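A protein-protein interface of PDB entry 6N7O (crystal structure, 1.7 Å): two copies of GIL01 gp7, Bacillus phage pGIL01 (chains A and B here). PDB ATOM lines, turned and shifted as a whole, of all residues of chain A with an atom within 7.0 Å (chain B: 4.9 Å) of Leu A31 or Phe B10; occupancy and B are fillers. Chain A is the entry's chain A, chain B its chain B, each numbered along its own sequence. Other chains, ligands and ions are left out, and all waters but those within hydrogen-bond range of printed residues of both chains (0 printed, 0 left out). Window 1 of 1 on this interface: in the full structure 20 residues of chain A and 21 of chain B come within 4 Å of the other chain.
Of the 14 printed residues of chain B, 6 touch a printed residue of chain A.
Hydrophobic or aromatic side chains of chain B within 4 Å of the printed part of chain A: Leu B7, Leu B8, Phe B10, Ile B11, Leu B14 and Leu B31.
Along chain A the printed residues that touch a printed residue of chain B span positions 10 to 35.
Among the printed residues, no Asp or Glu carboxylate lies within 4 Å of a Lys or Arg side-chain nitrogen of the other chain.
Phe A10 touches Leu B31, and with the chains exchanged Leu A31 touches Phe B10.
Leu A31 touches Leu B7, but with the chains exchanged Leu A7 does not touch Leu B31 (4.3 Å).
Leu B31 touches its own counterpart, Leu A31.
Val A34 touches Leu B7, but with the chains exchanged Leu A7 does not touch Val B34 (4.04 Å).
Positions printed for both chains: 7, 10, 26, 27, 30, 31 and 34.
Of the 12 pairs that touch across the chains among the printed residues, 3 have their exchanged pair printed and touching as well.
Leu A31 touches four residues of chain B.
Of the printed residues of chain A, Leu B7 touches Leu A31, Val A34 and Thr A35.
Of the printed residues of chain A, Leu B8 touches Thr A35 (3.9 Å).
Of chain A, only Leu A31 (3.6 Å) comes within 4 Å of Phe B10.
Of the printed residues of chain A, Ile B11 touches Leu A31, Met A32 and Thr A35.
Of the printed residues of chain A, Leu B31 touches Phe A10 (3.8 Å) and Leu A31 (3.8 Å).
The nearest residue of chain A that does not touch Phe B10 is Val A27 (4.9 Å).
The nearest printed residue of chain A that does not touch Leu B31 is Leu A7 (4.3 Å).
The backbone carbonyl oxygen (O) of Met A32 is in hydrogen-bond range of the side-chain hydroxyl (OG1) of Thr A35 (2.6 Å).
Among the printed residues, pairs that only touch across the chains: Thr A35 with Leu B7 (3.6 Å), Leu A31 with Phe B10 (3.6 Å), Val A27 with Leu B14 (3.6 Å), Thr A35 with Ile B11 (3.7 Å), Ile A28 with Leu B14 (3.7 Å), Leu A31 with Ile B11 (3.7 Å), Val A34 with Leu B7 (3.8 Å), Leu A31 with Leu B31 (3.8 Å), Phe A10 with Leu B31 (3.8 Å), Thr A35 with Leu B8 (3.9 Å), Leu A31 with Leu B7 (3.9 Å) and Met A32 with Ile B11 (3.96 Å).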
ATOM      1  N   MET A   3      12.378 -13.261 -30.634  1.00  0.00           N
ATOM      2  CA  MET A   3      13.473 -13.202 -29.664  1.00  0.00           C
ATOM      3  C   MET A   3      13.802 -11.763 -29.305  1.00  0.00           C
ATOM      4  O   MET A   3      14.019 -11.442 -28.132  1.00  0.00           O
ATOM      5  CB  MET A   3      14.735 -13.897 -30.193  1.00  0.00           C
ATOM      6  CG  MET A   3      16.005 -13.523 -29.397  1.00  0.00           C
ATOM      7  SD  MET A   3      17.542 -14.378 -29.848  1.00  0.00           S
ATOM      8  CE  MET A   3      17.029 -16.082 -29.683  1.00  0.00           C
ATOM      9  N   LEU A   7      13.359 -10.060 -25.565  1.00  0.00           N
ATOM     10  CA  LEU A   7      14.451  -9.406 -24.861  1.00  0.00           C
ATOM     11  C   LEU A   7      14.107  -7.962 -24.538  1.00  0.00           C
ATOM     12  O   LEU A   7      14.413  -7.482 -23.436  1.00  0.00           O
ATOM     13  CB  LEU A   7      15.728  -9.471 -25.686  1.00  0.00           C
ATOM     14  CG  LEU A   7      16.314 -10.870 -25.808  1.00  0.00           C
ATOM     15  CD1 LEU A   7      17.528 -10.821 -26.714  1.00  0.00           C
ATOM     16  CD2 LEU A   7      16.669 -11.412 -24.437  1.00  0.00           C
ATOM     17  N   PHE A  10      12.099  -7.961 -21.522  1.00  0.00           N
ATOM     18  CA  PHE A  10      12.893  -8.142 -20.316  1.00  0.00           C
ATOM     19  C   PHE A  10      13.618  -6.848 -19.952  1.00  0.00           C
ATOM     20  O   PHE A  10      13.683  -6.487 -18.768  1.00  0.00           O
ATOM     21  CB  PHE A  10      13.879  -9.302 -20.521  1.00  0.00           C
ATOM     22  CG  PHE A  10      14.604  -9.739 -19.265  1.00  0.00           C
ATOM     23  CD1 PHE A  10      13.988  -9.710 -18.019  1.00  0.00           C
ATOM     24  CD2 PHE A  10      15.907 -10.212 -19.340  1.00  0.00           C
ATOM     25  CE1 PHE A  10      14.669 -10.119 -16.870  1.00  0.00           C
ATOM     26  CE2 PHE A  10      16.582 -10.636 -18.193  1.00  0.00           C
ATOM     27  CZ  PHE A  10      15.968 -10.591 -16.960  1.00  0.00           C
ATOM     28  N   SER A  25      21.628 -15.624 -11.248  1.00  0.00           N
ATOM     29  CA  SER A  25      20.930 -16.843 -11.647  1.00  0.00           C
ATOM     30  C   SER A  25      19.563 -16.525 -12.241  1.00  0.00           C
ATOM     31  O   SER A  25      19.118 -17.205 -13.173  1.00  0.00           O
ATOM     32  CB  SER A  25      20.801 -17.803 -10.460  1.00  0.00           C
ATOM     33  OG  SER A  25      20.108 -17.205  -9.384  1.00  0.00           O
ATOM     34  N   TYR A  26      18.891 -15.489 -11.734  1.00  0.00           N
ATOM     35  CA  TYR A  26      17.604 -15.107 -12.301  1.00  0.00           C
ATOM     36  C   TYR A  26      17.754 -14.625 -13.731  1.00  0.00           C
ATOM     37  O   TYR A  26      16.955 -14.995 -14.605  1.00  0.00           O
ATOM     38  CB  TYR A  26      16.954 -14.023 -11.439  1.00  0.00           C
ATOM     39  CG  TYR A  26      15.716 -13.445 -12.070  1.00  0.00           C
ATOM     40  CD1 TYR A  26      14.546 -14.183 -12.138  1.00  0.00           C
ATOM     41  CD2 TYR A  26      15.725 -12.171 -12.626  1.00  0.00           C
ATOM     42  CE1 TYR A  26      13.404 -13.662 -12.727  1.00  0.00           C
ATOM     43  CE2 TYR A  26      14.591 -11.643 -13.221  1.00  0.00           C
ATOM     44  CZ  TYR A  26      13.433 -12.391 -13.268  1.00  0.00           C
ATOM     45  OH  TYR A  26      12.299 -11.879 -13.859  1.00  0.00           O
ATOM     46  N   VAL A  27      18.767 -13.787 -13.993  1.00  0.00           N
ATOM     47  CA  VAL A  27      18.980 -13.274 -15.343  1.00  0.00           C
ATOM     48  C   VAL A  27      19.284 -14.429 -16.284  1.00  0.00           C
ATOM     49  O   VAL A  27      18.709 -14.536 -17.373  1.00  0.00           O
ATOM     50  CB  VAL A  27      20.109 -12.221 -15.353  1.00  0.00           C
ATOM     51  CG1 VAL A  27      20.485 -11.812 -16.787  1.00  0.00           C
ATOM     52  CG2 VAL A  27      19.720 -10.990 -14.519  1.00  0.00           C
ATOM     53  N   ILE A  28      20.177 -15.328 -15.859  1.00  0.00           N
ATOM     54  CA  ILE A  28      20.565 -16.440 -16.721  1.00  0.00           C
ATOM     55  C   ILE A  28      19.355 -17.307 -17.041  1.00  0.00           C
ATOM     56  O   ILE A  28      19.127 -17.684 -18.201  1.00  0.00           O
ATOM     57  CB  ILE A  28      21.698 -17.249 -16.061  1.00  0.00           C
ATOM     58  CG1 ILE A  28      22.998 -16.433 -16.041  1.00  0.00           C
ATOM     59  CG2 ILE A  28      21.875 -18.589 -16.757  1.00  0.00           C
ATOM     60  CD1 ILE A  28      24.128 -17.107 -15.270  1.00  0.00           C
ATOM     61  N   ASP A  29      18.548 -17.613 -16.028  1.00  0.00           N
ATOM     62  CA  ASP A  29      17.357 -18.423 -16.266  1.00  0.00           C
ATOM     63  C   ASP A  29      16.414 -17.739 -17.249  1.00  0.00           C
ATOM     64  O   ASP A  29      15.878 -18.390 -18.157  1.00  0.00           O
ATOM     65  CB  ASP A  29      16.640 -18.719 -14.948  1.00  0.00           C
ATOM     66  CG  ASP A  29      17.347 -19.785 -14.116  1.00  0.00           C
ATOM     67  OD1 ASP A  29      18.283 -20.437 -14.627  1.00  0.00           O
ATOM     68  OD2 ASP A  29      16.946 -19.978 -12.947  1.00  0.00           O
ATOM     69  N   ARG A  30      16.194 -16.427 -17.089  1.00  0.00           N
ATOM     70  CA  ARG A  30      15.290 -15.715 -17.992  1.00  0.00           C
ATOM     71  C   ARG A  30      15.821 -15.734 -19.420  1.00  0.00           C
ATOM     72  O   ARG A  30      15.068 -15.986 -20.370  1.00  0.00           O
ATOM     73  CB  ARG A  30      15.085 -14.275 -17.512  1.00  0.00           C
ATOM     74  CG  ARG A  30      14.143 -14.125 -16.316  1.00  0.00           C
ATOM     75  CD  ARG A  30      12.712 -14.517 -16.664  1.00  0.00           C
ATOM     76  NE  ARG A  30      12.277 -13.976 -17.954  1.00  0.00           N
ATOM     77  CZ  ARG A  30      11.673 -12.803 -18.112  1.00  0.00           C
ATOM     78  NH1 ARG A  30      11.425 -12.038 -17.057  1.00  0.00           N
ATOM     79  NH2 ARG A  30      11.310 -12.397 -19.320  1.00  0.00           N
ATOM     80  N   LEU A  31      17.125 -15.462 -19.585  1.00  0.00           N
ATOM     81  CA  LEU A  31      17.719 -15.430 -20.917  1.00  0.00           C
ATOM     82  C   LEU A  31      17.727 -16.813 -21.564  1.00  0.00           C
ATOM     83  O   LEU A  31      17.524 -16.934 -22.781  1.00  0.00           O
ATOM     84  CB  LEU A  31      19.133 -14.861 -20.842  1.00  0.00           C
ATOM     85  CG  LEU A  31      19.165 -13.388 -20.405  1.00  0.00           C
ATOM     86  CD1 LEU A  31      20.609 -12.845 -20.388  1.00  0.00           C
ATOM     87  CD2 LEU A  31      18.271 -12.542 -21.302  1.00  0.00           C
ATOM     88  N   MET A  32      17.971 -17.863 -20.773  1.00  0.00           N
ATOM     89  CA  MET A  32      17.926 -19.215 -21.322  1.00  0.00           C
ATOM     90  C   MET A  32      16.547 -19.535 -21.864  1.00  0.00           C
ATOM     91  O   MET A  32      16.411 -20.217 -22.885  1.00  0.00           O
ATOM     92  CB  MET A  32      18.316 -20.249 -20.266  1.00  0.00           C
ATOM     93  CG  MET A  32      19.802 -20.495 -20.120  1.00  0.00           C
ATOM     94  SD  MET A  32      20.628 -21.091 -21.608  1.00  0.00           S
ATOM     95  CE  MET A  32      19.378 -22.111 -22.396  1.00  0.00           C
ATOM     96  N   GLN A  33      15.505 -19.061 -21.183  1.00  0.00           N
ATOM     97  CA  GLN A  33      14.153 -19.303 -21.668  1.00  0.00           C
ATOM     98  C   GLN A  33      13.975 -18.679 -23.047  1.00  0.00           C
ATOM     99  O   GLN A  33      13.331 -19.264 -23.923  1.00  0.00           O
ATOM    100  CB  GLN A  33      13.139 -18.753 -20.665  1.00  0.00           C
ATOM    101  CG  GLN A  33      11.818 -19.485 -20.642  1.00  0.00           C
ATOM    102  CD  GLN A  33      11.971 -20.916 -20.188  1.00  0.00           C
ATOM    103  OE1 GLN A  33      11.567 -21.844 -20.885  1.00  0.00           O
ATOM    104  NE2 GLN A  33      12.560 -21.104 -19.013  1.00  0.00           N
ATOM    105  N   VAL A  34      14.616 -17.530 -23.279  1.00  0.00           N
ATOM    106  CA  VAL A  34      14.493 -16.824 -24.553  1.00  0.00           C
ATOM    107  C   VAL A  34      15.199 -17.580 -25.682  1.00  0.00           C
ATOM    108  O   VAL A  34      14.763 -17.518 -26.838  1.00  0.00           O
ATOM    109  CB  VAL A  34      15.029 -15.385 -24.392  1.00  0.00           C
ATOM    110  CG1 VAL A  34      15.056 -14.653 -25.729  1.00  0.00           C
ATOM    111  CG2 VAL A  34      14.187 -14.610 -23.376  1.00  0.00           C
ATOM    112  N   THR A  35      16.283 -18.310 -25.381  1.00  0.00           N
ATOM    113  CA  THR A  35      17.029 -19.020 -26.419  1.00  0.00           C
ATOM    114  C   THR A  35      16.262 -20.188 -27.026  1.00  0.00           C
ATOM    115  O   THR A  35      16.715 -20.740 -28.034  1.00  0.00           O
ATOM    116  CB  THR A  35      18.359 -19.544 -25.870  1.00  0.00           C
ATOM    117  OG1 THR A  35      18.109 -20.532 -24.864  1.00  0.00           O
ATOM    118  CG2 THR A  35      19.181 -18.411 -25.273  1.00  0.00           C
ATOM    119  N   LYS A  36      15.138 -20.581 -26.441  1.00  0.00           N
ATOM    120  CA  LYS A  36      14.338 -21.672 -26.994  1.00  0.00           C
ATOM    121  C   LYS A  36      13.584 -21.227 -28.244  1.00  0.00           C
ATOM    122  O   LYS A  36      13.927 -21.622 -29.358  1.00  0.00           O
ATOM    123  CB  LYS A  36      13.359 -22.188 -25.949  1.00  0.00           C
ATOM    124  CG  LYS A  36      14.030 -22.613 -24.655  1.00  0.00           C
ATOM    125  CD  LYS A  36      13.018 -23.164 -23.666  1.00  0.00           C
ATOM    126  CE  LYS A  36      13.692 -23.612 -22.383  1.00  0.00           C
ATOM    127  NZ  LYS A  36      12.715 -24.211 -21.424  1.00  0.00           N
ATOM    128  N   LYS B   6      24.779 -14.013 -30.105  1.00  0.00           N
ATOM    129  CA  LYS B   6      25.175 -12.965 -29.168  1.00  0.00           C
ATOM    130  C   LYS B   6      24.505 -13.161 -27.820  1.00  0.00           C
ATOM    131  O   LYS B   6      25.112 -12.903 -26.772  1.00  0.00           O
ATOM    132  CB  LYS B   6      24.825 -11.584 -29.722  1.00  0.00           C
ATOM    133  CG  LYS B   6      25.617 -11.142 -30.919  1.00  0.00           C
ATOM    134  CD  LYS B   6      25.103  -9.793 -31.387  1.00  0.00           C
ATOM    135  CE  LYS B   6      25.916  -9.245 -32.529  1.00  0.00           C
ATOM    136  NZ  LYS B   6      25.488  -7.853 -32.834  1.00  0.00           N
ATOM    137  N   LEU B   7      23.245 -13.596 -27.822  1.00  0.00           N
ATOM    138  CA  LEU B   7      22.571 -13.853 -26.556  1.00  0.00           C
ATOM    139  C   LEU B   7      23.262 -14.975 -25.798  1.00  0.00           C
ATOM    140  O   LEU B   7      23.540 -14.850 -24.603  1.00  0.00           O
ATOM    141  CB  LEU B   7      21.096 -14.181 -26.803  1.00  0.00           C
ATOM    142  CG  LEU B   7      20.278 -14.520 -25.550  1.00  0.00           C
ATOM    143  CD1 LEU B   7      20.294 -13.346 -24.554  1.00  0.00           C
ATOM    144  CD2 LEU B   7      18.836 -14.879 -25.928  1.00  0.00           C
ATOM    145  N   LEU B   8      23.559 -16.085 -26.480  1.00  0.00           N
ATOM    146  CA  LEU B   8      24.256 -17.183 -25.819  1.00  0.00           C
ATOM    147  C   LEU B   8      25.619 -16.741 -25.287  1.00  0.00           C
ATOM    148  O   LEU B   8      26.018 -17.143 -24.188  1.00  0.00           O
ATOM    149  CB  LEU B   8      24.390 -18.363 -26.777  1.00  0.00           C
ATOM    150  CG  LEU B   8      23.098 -19.184 -26.888  1.00  0.00           C
ATOM    151  CD1 LEU B   8      23.162 -20.234 -27.983  1.00  0.00           C
ATOM    152  CD2 LEU B   8      22.747 -19.839 -25.544  1.00  0.00           C
ATOM    153  N   ASP B   9      26.339 -15.899 -26.035  1.00  0.00           N
ATOM    154  CA  ASP B   9      27.626 -15.425 -25.527  1.00  0.00           C
ATOM    155  C   ASP B   9      27.462 -14.549 -24.288  1.00  0.00           C
ATOM    156  O   ASP B   9      28.319 -14.580 -23.393  1.00  0.00           O
ATOM    157  CB  ASP B   9      28.407 -14.687 -26.621  1.00  0.00           C
ATOM    158  CG  ASP B   9      29.084 -15.647 -27.602  1.00  0.00           C
ATOM    159  OD1 ASP B   9      29.174 -16.854 -27.298  1.00  0.00           O
ATOM    160  OD2 ASP B   9      29.532 -15.203 -28.679  1.00  0.00           O
ATOM    161  N   PHE B  10      26.369 -13.772 -24.195  1.00  0.00           N
ATOM    162  CA  PHE B  10      26.124 -13.018 -22.970  1.00  0.00           C
ATOM    163  C   PHE B  10      25.807 -13.959 -21.820  1.00  0.00           C
ATOM    164  O   PHE B  10      26.304 -13.769 -20.705  1.00  0.00           O
ATOM    165  CB  PHE B  10      24.988 -12.008 -23.180  1.00  0.00           C
ATOM    166  CG  PHE B  10      24.684 -11.163 -21.967  1.00  0.00           C
ATOM    167  CD1 PHE B  10      25.706 -10.651 -21.174  1.00  0.00           C
ATOM    168  CD2 PHE B  10      23.371 -10.855 -21.634  1.00  0.00           C
ATOM    169  CE1 PHE B  10      25.418  -9.851 -20.074  1.00  0.00           C
ATOM    170  CE2 PHE B  10      23.078 -10.051 -20.540  1.00  0.00           C
ATOM    171  CZ  PHE B  10      24.097  -9.556 -19.747  1.00  0.00           C
ATOM    172  N   ILE B  11      25.013 -15.003 -22.077  1.00  0.00           N
ATOM    173  CA  ILE B  11      24.751 -16.000 -21.042  1.00  0.00           C
ATOM    174  C   ILE B  11      26.055 -16.622 -20.552  1.00  0.00           C
ATOM    175  O   ILE B  11      26.241 -16.849 -19.346  1.00  0.00           O
ATOM    176  CB  ILE B  11      23.774 -17.067 -21.568  1.00  0.00           C
ATOM    177  CG1 ILE B  11      22.392 -16.453 -21.773  1.00  0.00           C
ATOM    178  CG2 ILE B  11      23.680 -18.242 -20.611  1.00  0.00           C
ATOM    179  CD1 ILE B  11      21.446 -17.337 -22.590  1.00  0.00           C
ATOM    180  N   ILE B  12      26.974 -16.918 -21.471  1.00  0.00           N
ATOM    181  CA  ILE B  12      28.268 -17.477 -21.074  1.00  0.00           C
ATOM    182  C   ILE B  12      29.042 -16.465 -20.234  1.00  0.00           C
ATOM    183  O   ILE B  12      29.651 -16.822 -19.214  1.00  0.00           O
ATOM    184  CB  ILE B  12      29.068 -17.915 -22.314  1.00  0.00           C
ATOM    185  CG1 ILE B  12      28.353 -19.063 -23.021  1.00  0.00           C
ATOM    186  CG2 ILE B  12      30.495 -18.356 -21.926  1.00  0.00           C
ATOM    187  CD1 ILE B  12      28.884 -19.329 -24.387  1.00  0.00           C
ATOM    188  N   GLU B  13      29.038 -15.193 -20.654  1.00  0.00           N
ATOM    189  CA  GLU B  13      29.713 -14.154 -19.879  1.00  0.00           C
ATOM    190  C   GLU B  13      29.203 -14.101 -18.443  1.00  0.00           C
ATOM    191  O   GLU B  13      29.993 -13.933 -17.509  1.00  0.00           O
ATOM    192  CB  GLU B  13      29.549 -12.788 -20.558  1.00  0.00           C
ATOM    193  CG  GLU B  13      30.263 -11.671 -19.816  1.00  0.00           C
ATOM    194  CD  GLU B  13      29.925 -10.274 -20.350  1.00  0.00           C
ATOM    195  OE1 GLU B  13      30.382  -9.300 -19.735  1.00  0.00           O
ATOM    196  OE2 GLU B  13      29.212 -10.153 -21.377  1.00  0.00           O
ATOM    197  N   LEU B  14      27.882 -14.209 -18.242  1.00  0.00           N
ATOM    198  CA  LEU B  14      27.350 -14.260 -16.885  1.00  0.00           C
ATOM    199  C   LEU B  14      27.769 -15.544 -16.180  1.00  0.00           C
ATOM    200  O   LEU B  14      28.254 -15.517 -15.043  1.00  0.00           O
ATOM    201  CB  LEU B  14      25.821 -14.137 -16.923  1.00  0.00           C
ATOM    202  CG  LEU B  14      25.279 -12.837 -17.513  1.00  0.00           C
ATOM    203  CD1 LEU B  14      23.784 -12.935 -17.823  1.00  0.00           C
ATOM    204  CD2 LEU B  14      25.545 -11.667 -16.574  1.00  0.00           C
ATOM    205  N   TYR B  26      24.277  -2.742 -16.153  1.00  0.00           N
ATOM    206  CA  TYR B  26      25.139  -3.509 -17.047  1.00  0.00           C
ATOM    207  C   TYR B  26      24.340  -4.529 -17.852  1.00  0.00           C
ATOM    208  O   TYR B  26      24.560  -4.679 -19.060  1.00  0.00           O
ATOM    209  CB  TYR B  26      26.244  -4.222 -16.269  1.00  0.00           C
ATOM    210  CG  TYR B  26      27.199  -4.942 -17.199  1.00  0.00           C
ATOM    211  CD1 TYR B  26      28.023  -4.224 -18.050  1.00  0.00           C
ATOM    212  CD2 TYR B  26      27.259  -6.327 -17.242  1.00  0.00           C
ATOM    213  CE1 TYR B  26      28.895  -4.860 -18.916  1.00  0.00           C
ATOM    214  CE2 TYR B  26      28.132  -6.980 -18.105  1.00  0.00           C
ATOM    215  CZ  TYR B  26      28.952  -6.238 -18.940  1.00  0.00           C
ATOM    216  OH  TYR B  26      29.835  -6.857 -19.804  1.00  0.00           O
ATOM    217  N   VAL B  27      23.441  -5.270 -17.192  1.00  0.00           N
ATOM    218  CA  VAL B  27      22.613  -6.242 -17.912  1.00  0.00           C
ATOM    219  C   VAL B  27      21.822  -5.542 -19.009  1.00  0.00           C
ATOM    220  O   VAL B  27      21.750  -6.012 -20.149  1.00  0.00           O
ATOM    221  CB  VAL B  27      21.680  -6.996 -16.943  1.00  0.00           C
ATOM    222  CG1 VAL B  27      20.677  -7.861 -17.690  1.00  0.00           C
ATOM    223  CG2 VAL B  27      22.496  -7.862 -15.972  1.00  0.00           C
ATOM    224  N   ARG B  30      24.052  -4.579 -21.926  1.00  0.00           N
ATOM    225  CA  ARG B  30      24.460  -5.714 -22.756  1.00  0.00           C
ATOM    226  C   ARG B  30      23.310  -6.216 -23.624  1.00  0.00           C
ATOM    227  O   ARG B  30      23.516  -6.580 -24.793  1.00  0.00           O
ATOM    228  CB  ARG B  30      24.998  -6.847 -21.886  1.00  0.00           C
ATOM    229  CG  ARG B  30      26.299  -6.499 -21.187  1.00  0.00           C
ATOM    230  CD  ARG B  30      27.498  -6.558 -22.127  1.00  0.00           C
ATOM    231  NE  ARG B  30      27.821  -7.936 -22.505  1.00  0.00           N
ATOM    232  CZ  ARG B  30      27.637  -8.431 -23.726  1.00  0.00           C
ATOM    233  NH1 ARG B  30      27.133  -7.660 -24.677  1.00  0.00           N
ATOM    234  NH2 ARG B  30      27.955  -9.693 -24.001  1.00  0.00           N
ATOM    235  N   LEU B  31      22.098  -6.272 -23.065  1.00  0.00           N
ATOM    236  CA  LEU B  31      20.956  -6.743 -23.841  1.00  0.00           C
ATOM    237  C   LEU B  31      20.618  -5.761 -24.959  1.00  0.00           C
ATOM    238  O   LEU B  31      20.196  -6.172 -26.045  1.00  0.00           O
ATOM    239  CB  LEU B  31      19.751  -6.967 -22.929  1.00  0.00           C
ATOM    240  CG  LEU B  31      19.890  -8.117 -21.924  1.00  0.00           C
ATOM    241  CD1 LEU B  31      18.705  -8.179 -21.001  1.00  0.00           C
ATOM    242  CD2 LEU B  31      20.050  -9.437 -22.679  1.00  0.00           C
ATOM    243  N   VAL B  34      22.882  -6.740 -27.563  1.00  0.00           N
ATOM    244  CA  VAL B  34      22.485  -7.996 -28.198  1.00  0.00           C
ATOM    245  C   VAL B  34      21.378  -7.759 -29.216  1.00  0.00           C
ATOM    246  O   VAL B  34      21.374  -8.352 -30.307  1.00  0.00           O
ATOM    247  CB  VAL B  34      22.055  -9.008 -27.124  1.00  0.00           C
ATOM    248  CG1 VAL B  34      21.377 -10.210 -27.774  1.00  0.00           C
ATOM    249  CG2 VAL B  34      23.259  -9.432 -26.292  1.00  0.00           C
